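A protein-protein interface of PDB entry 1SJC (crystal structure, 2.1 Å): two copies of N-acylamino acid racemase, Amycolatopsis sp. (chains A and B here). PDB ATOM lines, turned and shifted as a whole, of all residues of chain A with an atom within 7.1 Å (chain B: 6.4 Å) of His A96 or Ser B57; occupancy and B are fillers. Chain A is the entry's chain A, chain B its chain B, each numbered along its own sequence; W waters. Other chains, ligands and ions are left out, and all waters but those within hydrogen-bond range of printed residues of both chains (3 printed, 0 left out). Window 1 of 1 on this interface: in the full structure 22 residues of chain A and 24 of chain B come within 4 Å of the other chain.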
ATOM      1  N   SER A  57       8.284 -15.681  12.310  1.00  0.00           N
ATOM      2  CA  SER A  57       7.079 -15.000  11.903  1.00  0.00           C
ATOM      3  C   SER A  57       7.266 -13.532  11.682  1.00  0.00           C
ATOM      4  O   SER A  57       6.347 -12.872  11.207  1.00  0.00           O
ATOM      5  CB  SER A  57       6.000 -15.220  12.914  1.00  0.00           C
ATOM      6  OG  SER A  57       6.294 -14.482  14.076  1.00  0.00           O
ATOM      7  N   GLU A  58       8.452 -13.029  12.048  1.00  0.00           N
ATOM      8  CA  GLU A  58       8.751 -11.611  11.919  1.00  0.00           C
ATOM      9  C   GLU A  58       9.320 -11.232  10.569  1.00  0.00           C
ATOM     10  O   GLU A  58      10.069 -11.988   9.952  1.00  0.00           O
ATOM     11  CB  GLU A  58       9.656 -11.093  13.027  1.00  0.00           C
ATOM     12  CG  GLU A  58       8.893 -10.738  14.310  1.00  0.00           C
ATOM     13  CD  GLU A  58       9.816 -10.320  15.441  1.00  0.00           C
ATOM     14  OE1 GLU A  58      10.322 -11.090  16.234  1.00  0.00           O
ATOM     15  OE2 GLU A  58      10.030  -9.040  15.520  1.00  0.00           O
ATOM     16  N   GLY A  62       6.517  -5.886   8.960  1.00  0.00           N
ATOM     17  CA  GLY A  62       5.851  -6.179  10.223  1.00  0.00           C
ATOM     18  C   GLY A  62       6.481  -5.425  11.375  1.00  0.00           C
ATOM     19  O   GLY A  62       5.780  -4.782  12.186  1.00  0.00           O
ATOM     20  N   ALA A  63       7.817  -5.491  11.405  1.00  0.00           N
ATOM     21  CA  ALA A  63       8.592  -4.821  12.434  1.00  0.00           C
ATOM     22  C   ALA A  63       8.395  -3.319  12.382  1.00  0.00           C
ATOM     23  O   ALA A  63       8.186  -2.611  13.388  1.00  0.00           O
ATOM     24  CB  ALA A  63      10.042  -5.145  12.223  1.00  0.00           C
ATOM     25  N   VAL A  66       5.043  -2.335  13.795  1.00  0.00           N
ATOM     26  CA  VAL A  66       4.882  -2.350  15.233  1.00  0.00           C
ATOM     27  C   VAL A  66       5.742  -1.294  15.928  1.00  0.00           C
ATOM     28  O   VAL A  66       5.359  -0.653  16.914  1.00  0.00           O
ATOM     29  CB  VAL A  66       5.161  -3.740  15.757  1.00  0.00           C
ATOM     30  CG1 VAL A  66       6.667  -3.963  15.887  1.00  0.00           C
ATOM     31  CG2 VAL A  66       4.450  -3.930  17.086  1.00  0.00           C
ATOM     32  N   LEU A  67       6.933  -1.106  15.403  1.00  0.00           N
ATOM     33  CA  LEU A  67       7.809  -0.148  16.030  1.00  0.00           C
ATOM     34  C   LEU A  67       7.174   1.197  16.069  1.00  0.00           C
ATOM     35  O   LEU A  67       7.087   1.883  17.086  1.00  0.00           O
ATOM     36  CB  LEU A  67       9.081  -0.051  15.204  1.00  0.00           C
ATOM     37  CG  LEU A  67      10.087  -1.101  15.628  1.00  0.00           C
ATOM     38  CD1 LEU A  67      10.936  -1.538  14.446  1.00  0.00           C
ATOM     39  CD2 LEU A  67      10.957  -0.534  16.736  1.00  0.00           C
ATOM     40  N   LEU A  71       5.753   0.347  19.504  1.00  0.00           N
ATOM     41  CA  LEU A  71       6.937   0.412  20.285  1.00  0.00           C
ATOM     42  C   LEU A  71       7.629   1.731  20.422  1.00  0.00           C
ATOM     43  O   LEU A  71       8.000   2.098  21.542  1.00  0.00           O
ATOM     44  CB  LEU A  71       7.900  -0.679  19.911  1.00  0.00           C
ATOM     45  CG  LEU A  71       7.279  -2.048  19.697  1.00  0.00           C
ATOM     46  CD1 LEU A  71       8.419  -2.931  19.222  1.00  0.00           C
ATOM     47  CD2 LEU A  71       6.639  -2.648  20.960  1.00  0.00           C
ATOM     48  N   PHE A  93       3.207  -5.425  24.937  1.00  0.00           N
ATOM     49  CA  PHE A  93       3.100  -5.927  23.580  1.00  0.00           C
ATOM     50  C   PHE A  93       3.751  -7.278  23.507  1.00  0.00           C
ATOM     51  O   PHE A  93       4.950  -7.452  23.776  1.00  0.00           O
ATOM     52  CB  PHE A  93       3.796  -4.977  22.593  1.00  0.00           C
ATOM     53  CG  PHE A  93       3.353  -3.589  22.896  1.00  0.00           C
ATOM     54  CD1 PHE A  93       4.274  -2.670  23.391  1.00  0.00           C
ATOM     55  CD2 PHE A  93       2.016  -3.209  22.749  1.00  0.00           C
ATOM     56  CE1 PHE A  93       3.866  -1.367  23.689  1.00  0.00           C
ATOM     57  CE2 PHE A  93       1.596  -1.910  23.041  1.00  0.00           C
ATOM     58  CZ  PHE A  93       2.530  -0.993  23.522  1.00  0.00           C
ATOM     59  N   LYS A  94       2.937  -8.230  23.130  1.00  0.00           N
ATOM     60  CA  LYS A  94       3.382  -9.607  23.004  1.00  0.00           C
ATOM     61  C   LYS A  94       4.174  -9.841  21.749  1.00  0.00           C
ATOM     62  O   LYS A  94       3.749  -9.371  20.685  1.00  0.00           O
ATOM     63  CB  LYS A  94       2.176 -10.543  22.979  1.00  0.00           C
ATOM     64  CG  LYS A  94       1.222 -10.290  24.143  1.00  0.00           C
ATOM     65  CD  LYS A  94       1.630 -11.087  25.379  1.00  0.00           C
ATOM     66  CE  LYS A  94       0.585 -11.041  26.483  1.00  0.00           C
ATOM     67  NZ  LYS A  94       0.954 -11.752  27.716  1.00  0.00           N
ATOM     68  N   GLY A  95       5.289 -10.592  21.915  1.00  0.00           N
ATOM     69  CA  GLY A  95       6.177 -10.994  20.826  1.00  0.00           C
ATOM     70  C   GLY A  95       7.000  -9.839  20.306  1.00  0.00           C
ATOM     71  O   GLY A  95       7.404  -8.998  21.081  1.00  0.00           O
ATOM     72  N   HIS A  96       7.243  -9.828  19.002  1.00  0.00           N
ATOM     73  CA  HIS A  96       7.977  -8.767  18.325  1.00  0.00           C
ATOM     74  C   HIS A  96       9.357  -8.526  18.861  1.00  0.00           C
ATOM     75  O   HIS A  96       9.817  -7.378  18.934  1.00  0.00           O
ATOM     76  CB  HIS A  96       7.161  -7.465  18.221  1.00  0.00           C
ATOM     77  CG  HIS A  96       5.842  -7.740  17.547  1.00  0.00           C
ATOM     78  ND1 HIS A  96       5.739  -7.817  16.159  1.00  0.00           N
ATOM     79  CD2 HIS A  96       4.597  -7.998  18.085  1.00  0.00           C
ATOM     80  CE1 HIS A  96       4.466  -8.111  15.884  1.00  0.00           C
ATOM     81  NE2 HIS A  96       3.748  -8.218  17.016  1.00  0.00           N
ATOM     82  N   ARG A  97       9.993  -9.644  19.199  1.00  0.00           N
ATOM     83  CA  ARG A  97      11.340  -9.659  19.709  1.00  0.00           C
ATOM     84  C   ARG A  97      12.377  -9.062  18.776  1.00  0.00           C
ATOM     85  O   ARG A  97      13.214  -8.334  19.269  1.00  0.00           O
ATOM     86  CB  ARG A  97      11.758 -11.069  19.992  1.00  0.00           C
ATOM     87  CG  ARG A  97      11.000 -11.620  21.173  1.00  0.00           C
ATOM     88  CD  ARG A  97      11.520 -13.015  21.531  1.00  0.00           C
ATOM     89  NE  ARG A  97      10.982 -13.456  22.806  1.00  0.00           N
ATOM     90  CZ  ARG A  97       9.864 -14.177  22.957  1.00  0.00           C
ATOM     91  NH1 ARG A  97       9.111 -14.626  21.942  1.00  0.00           N
ATOM     92  NH2 ARG A  97       9.485 -14.453  24.191  1.00  0.00           N
ATOM     93  N   MET A  98      12.396  -9.401  17.473  1.00  0.00           N
ATOM     94  CA  MET A  98      13.428  -8.793  16.662  1.00  0.00           C
ATOM     95  C   MET A  98      13.336  -7.285  16.707  1.00  0.00           C
ATOM     96  O   MET A  98      14.314  -6.587  16.903  1.00  0.00           O
ATOM     97  CB  MET A  98      13.672  -9.310  15.244  1.00  0.00           C
ATOM     98  CG  MET A  98      13.022 -10.629  14.990  1.00  0.00           C
ATOM     99  SD  MET A  98      13.976 -11.740  13.970  1.00  0.00           S
ATOM    100  CE  MET A  98      12.724 -12.292  12.794  1.00  0.00           C
ATOM    101  N   ALA A  99      12.131  -6.796  16.546  1.00  0.00           N
ATOM    102  CA  ALA A  99      11.889  -5.372  16.562  1.00  0.00           C
ATOM    103  C   ALA A  99      12.305  -4.785  17.892  1.00  0.00           C
ATOM    104  O   ALA A  99      13.108  -3.859  17.960  1.00  0.00           O
ATOM    105  CB  ALA A  99      10.416  -5.068  16.291  1.00  0.00           C
ATOM    106  N   LYS A 100      11.729  -5.325  18.957  1.00  0.00           N
ATOM    107  CA  LYS A 100      12.048  -4.862  20.290  1.00  0.00           C
ATOM    108  C   LYS A 100      13.567  -4.807  20.523  1.00  0.00           C
ATOM    109  O   LYS A 100      14.057  -3.888  21.177  1.00  0.00           O
ATOM    110  CB  LYS A 100      11.403  -5.759  21.334  1.00  0.00           C
ATOM    111  CG  LYS A 100       9.955  -5.439  21.693  1.00  0.00           C
ATOM    112  CD  LYS A 100       9.390  -6.420  22.734  1.00  0.00           C
ATOM    113  CE  LYS A 100       7.928  -6.187  23.203  1.00  0.00           C
ATOM    114  NZ  LYS A 100       7.435  -7.087  24.296  1.00  0.00           N
ATOM    115  N   GLY A 101      14.299  -5.806  19.982  1.00  0.00           N
ATOM    116  CA  GLY A 101      15.757  -5.962  20.123  1.00  0.00           C
ATOM    117  C   GLY A 101      16.568  -4.880  19.439  1.00  0.00           C
ATOM    118  O   GLY A 101      17.593  -4.441  19.933  1.00  0.00           O
ATOM    119  N   ALA A 102      16.065  -4.455  18.297  1.00  0.00           N
ATOM    120  CA  ALA A 102      16.671  -3.426  17.502  1.00  0.00           C
ATOM    121  C   ALA A 102      16.606  -2.116  18.261  1.00  0.00           C
ATOM    122  O   ALA A 102      17.564  -1.352  18.417  1.00  0.00           O
ATOM    123  CB  ALA A 102      15.851  -3.330  16.211  1.00  0.00           C
ATOM    124  N   GLY A 265      18.821 -10.467  18.374  1.00  0.00           N
ATOM    125  CA  GLY A 265      17.546  -9.972  17.787  1.00  0.00           C
ATOM    126  C   GLY A 265      16.410 -10.943  18.072  1.00  0.00           C
ATOM    127  O   GLY A 265      15.344 -10.574  18.553  1.00  0.00           O
ATOM    128  N   GLY A 268      15.241 -10.820  21.500  1.00  0.00           N
ATOM    129  CA  GLY A 268      14.681  -9.530  21.938  1.00  0.00           C
ATOM    130  C   GLY A 268      15.695  -8.504  22.516  1.00  0.00           C
ATOM    131  O   GLY A 268      15.346  -7.581  23.267  1.00  0.00           O
ATOM    132  N   GLY B  52      -4.499  -4.029  18.826  1.00  0.00           N
ATOM    133  CA  GLY B  52      -3.096  -4.138  19.202  1.00  0.00           C
ATOM    134  C   GLY B  52      -2.808  -5.554  19.652  1.00  0.00           C
ATOM    135  O   GLY B  52      -3.693  -6.382  19.854  1.00  0.00           O
ATOM    136  N   PRO B  53      -1.541  -5.806  19.804  1.00  0.00           N
ATOM    137  CA  PRO B  53      -1.013  -7.115  20.147  1.00  0.00           C
ATOM    138  C   PRO B  53      -0.940  -7.338  21.615  1.00  0.00           C
ATOM    139  O   PRO B  53       0.140  -7.417  22.170  1.00  0.00           O
ATOM    140  CB  PRO B  53       0.392  -7.097  19.601  1.00  0.00           C
ATOM    141  CG  PRO B  53       0.742  -5.623  19.368  1.00  0.00           C
ATOM    142  CD  PRO B  53      -0.565  -4.871  19.207  1.00  0.00           C
ATOM    143  N   LEU B  54      -2.078  -7.447  22.258  1.00  0.00           N
ATOM    144  CA  LEU B  54      -2.057  -7.599  23.686  1.00  0.00           C
ATOM    145  C   LEU B  54      -2.319  -8.954  24.244  1.00  0.00           C
ATOM    146  O   LEU B  54      -1.782  -9.206  25.309  1.00  0.00           O
ATOM    147  CB  LEU B  54      -2.938  -6.586  24.381  1.00  0.00           C
ATOM    148  CG  LEU B  54      -2.716  -5.185  23.852  1.00  0.00           C
ATOM    149  CD1 LEU B  54      -3.561  -4.269  24.687  1.00  0.00           C
ATOM    150  CD2 LEU B  54      -1.274  -4.761  24.054  1.00  0.00           C
ATOM    151  N   TYR B  55      -3.160  -9.769  23.597  1.00  0.00           N
ATOM    152  CA  TYR B  55      -3.442 -11.124  24.086  1.00  0.00           C
ATOM    153  C   TYR B  55      -2.338 -12.033  23.514  1.00  0.00           C
ATOM    154  O   TYR B  55      -1.912 -13.034  24.096  1.00  0.00           O
ATOM    155  CB  TYR B  55      -4.894 -11.599  23.701  1.00  0.00           C
ATOM    156  CG  TYR B  55      -5.120 -13.116  23.567  1.00  0.00           C
ATOM    157  CD1 TYR B  55      -4.774 -13.784  22.387  1.00  0.00           C
ATOM    158  CD2 TYR B  55      -5.733 -13.858  24.587  1.00  0.00           C
ATOM    159  CE1 TYR B  55      -4.981 -15.160  22.251  1.00  0.00           C
ATOM    160  CE2 TYR B  55      -5.962 -15.232  24.460  1.00  0.00           C
ATOM    161  CZ  TYR B  55      -5.571 -15.887  23.286  1.00  0.00           C
ATOM    162  OH  TYR B  55      -5.737 -17.248  23.161  1.00  0.00           O
ATOM    163  N   SER B  56      -1.876 -11.610  22.339  1.00  0.00           N
ATOM    164  CA  SER B  56      -0.843 -12.273  21.588  1.00  0.00           C
ATOM    165  C   SER B  56      -0.194 -11.276  20.641  1.00  0.00           C
ATOM    166  O   SER B  56      -0.634 -10.100  20.566  1.00  0.00           O
ATOM    167  CB  SER B  56      -1.394 -13.482  20.829  1.00  0.00           C
ATOM    168  OG  SER B  56      -2.141 -13.079  19.691  1.00  0.00           O
ATOM    169  N   SER B  57       0.820 -11.777  19.901  1.00  0.00           N
ATOM    170  CA  SER B  57       1.583 -10.971  18.959  1.00  0.00           C
ATOM    171  C   SER B  57       0.788 -10.418  17.791  1.00  0.00           C
ATOM    172  O   SER B  57       1.142  -9.364  17.253  1.00  0.00           O
ATOM    173  CB  SER B  57       2.857 -11.633  18.442  1.00  0.00           C
ATOM    174  OG  SER B  57       2.528 -12.731  17.607  1.00  0.00           O
ATOM    175  N   GLU B  58      -0.267 -11.124  17.400  1.00  0.00           N
ATOM    176  CA  GLU B  58      -1.111 -10.727  16.266  1.00  0.00           C
ATOM    177  C   GLU B  58      -2.051  -9.586  16.524  1.00  0.00           C
ATOM    178  O   GLU B  58      -2.576  -9.394  17.620  1.00  0.00           O
ATOM    179  CB  GLU B  58      -1.859 -11.923  15.633  1.00  0.00           C
ATOM    180  CG  GLU B  58      -0.852 -13.010  15.167  1.00  0.00           C
ATOM    181  CD  GLU B  58      -1.558 -14.125  14.494  1.00  0.00           C
ATOM    182  OE1 GLU B  58      -1.828 -15.157  15.037  1.00  0.00           O
ATOM    183  OE2 GLU B  58      -1.913 -13.822  13.284  1.00  0.00           O
ATOM    184  N   TYR B  59      -2.255  -8.815  15.482  1.00  0.00           N
ATOM    185  CA  TYR B  59      -3.168  -7.702  15.579  1.00  0.00           C
ATOM    186  C   TYR B  59      -3.719  -7.341  14.208  1.00  0.00           C
ATOM    187  O   TYR B  59      -3.107  -7.608  13.149  1.00  0.00           O
ATOM    188  CB  TYR B  59      -2.629  -6.505  16.380  1.00  0.00           C
ATOM    189  CG  TYR B  59      -1.405  -5.874  15.753  1.00  0.00           C
ATOM    190  CD1 TYR B  59      -0.142  -6.475  15.847  1.00  0.00           C
ATOM    191  CD2 TYR B  59      -1.537  -4.664  15.065  1.00  0.00           C
ATOM    192  CE1 TYR B  59       0.989  -5.859  15.299  1.00  0.00           C
ATOM    193  CE2 TYR B  59      -0.412  -4.055  14.500  1.00  0.00           C
ATOM    194  CZ  TYR B  59       0.853  -4.640  14.615  1.00  0.00           C
ATOM    195  OH  TYR B  59       1.955  -3.971  14.062  1.00  0.00           O
ATOM    196  N   GLU B 219       2.360 -17.281  28.076  1.00  0.00           N
ATOM    197  CA  GLU B 219       2.141 -18.239  27.007  1.00  0.00           C
ATOM    198  C   GLU B 219       3.264 -19.263  26.813  1.00  0.00           C
ATOM    199  O   GLU B 219       3.055 -20.439  26.499  1.00  0.00           O
ATOM    200  CB  GLU B 219       1.884 -17.488  25.682  1.00  0.00           C
ATOM    201  CG  GLU B 219       2.082 -18.356  24.414  1.00  0.00           C
ATOM    202  CD  GLU B 219       2.027 -17.500  23.182  1.00  0.00           C
ATOM    203  OE1 GLU B 219       1.433 -16.417  23.116  1.00  0.00           O
ATOM    204  OE2 GLU B 219       2.729 -18.039  22.220  1.00  0.00           O
HETATM  205  O   HOH W   1      -2.280 -10.799  28.352  1.00  0.00           O
HETATM  206  O   HOH W   2       3.381  -5.755  12.434  1.00  0.00           O
HETATM  207  O   HOH W   3       2.193 -14.594  27.066  1.00  0.00           O
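Positions printed for both chains: 57 and 58. Of the 9 pairs that touch across the chains among the printed residues, none has its exchanged pair printed and touching as well.
Printed residues of chain B within 4 Å of Val A66: Tyr B59 (3.5 Å). Of the printed residues of chain B, Phe A93 touches Pro B53 (3.6 Å) and Leu B54 (3.9 Å). Of the printed residues of chain B, His A96 touches Ser B57 (2.9 Å). Met A98 touches none of the printed residues of chain B. Of chain A, only Lys A94 (3.2 Å) and His A96 (2.9 Å) come within 4 Å of Ser B57. The nearest printed residue of chain B that does not touch His A96 is Tyr B59 (4.02 Å). The nearest residue of chain A that does not touch Ser B57 is Gly A95 (4.1 Å).
The backbone carbonyl oxygen of Phe A93 sits at hydrogen-bond distance from the side-chain amino group of Lys A100 (2.6 Å). The backbone carbonyl oxygen (O) of Val A66 is in hydrogen-bond range of the backbone NH (N) of Leu A71, at 2.8 Å.
OH of Tyr B59 touches N of Val A66 (3.5 Å). Phe A93 touches Pro B53. CD2 of Phe A93 touches CD2 of Leu B54 (3.9 Å). Lys A94 touches Leu B54 (CE to O, 3.2 Å). Lys A94 touches Tyr B55 (CE to O, 3.99 Å). Lys A94 touches Ser B56 (CB to C, 3.4 Å). CA of Ser B57 touches O of Lys A94 (3.2 Å).
The backbone NH of Lys A94 sits at hydrogen-bond distance from the backbone carbonyl oxygen of Pro B53 (3.1 Å). NE2 of His A96 is in hydrogen-bond range of O of Ser B57 (2.9 Å).
Water W2 bridges O of Gly A62 (2.6 Å) and OH of Tyr B59 (2.8 Å). Water W3 lies within hydrogen-bond range of the backbone NH of Glu B219 (2.9 Å) and the side-chain amino group of Lys A94 (3.2 Å). Water W1 bridges NZ of Lys A94 and O of Leu B54.
Of the 19 printed residues of chain A, 4 touch a printed residue of chain B. Among the printed residues, 9 pairs touch across the chains. Among the printed residues, no Asp or Glu carboxylate lies within 4 Å of a Lys or Arg side-chain nitrogen of the other chain.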
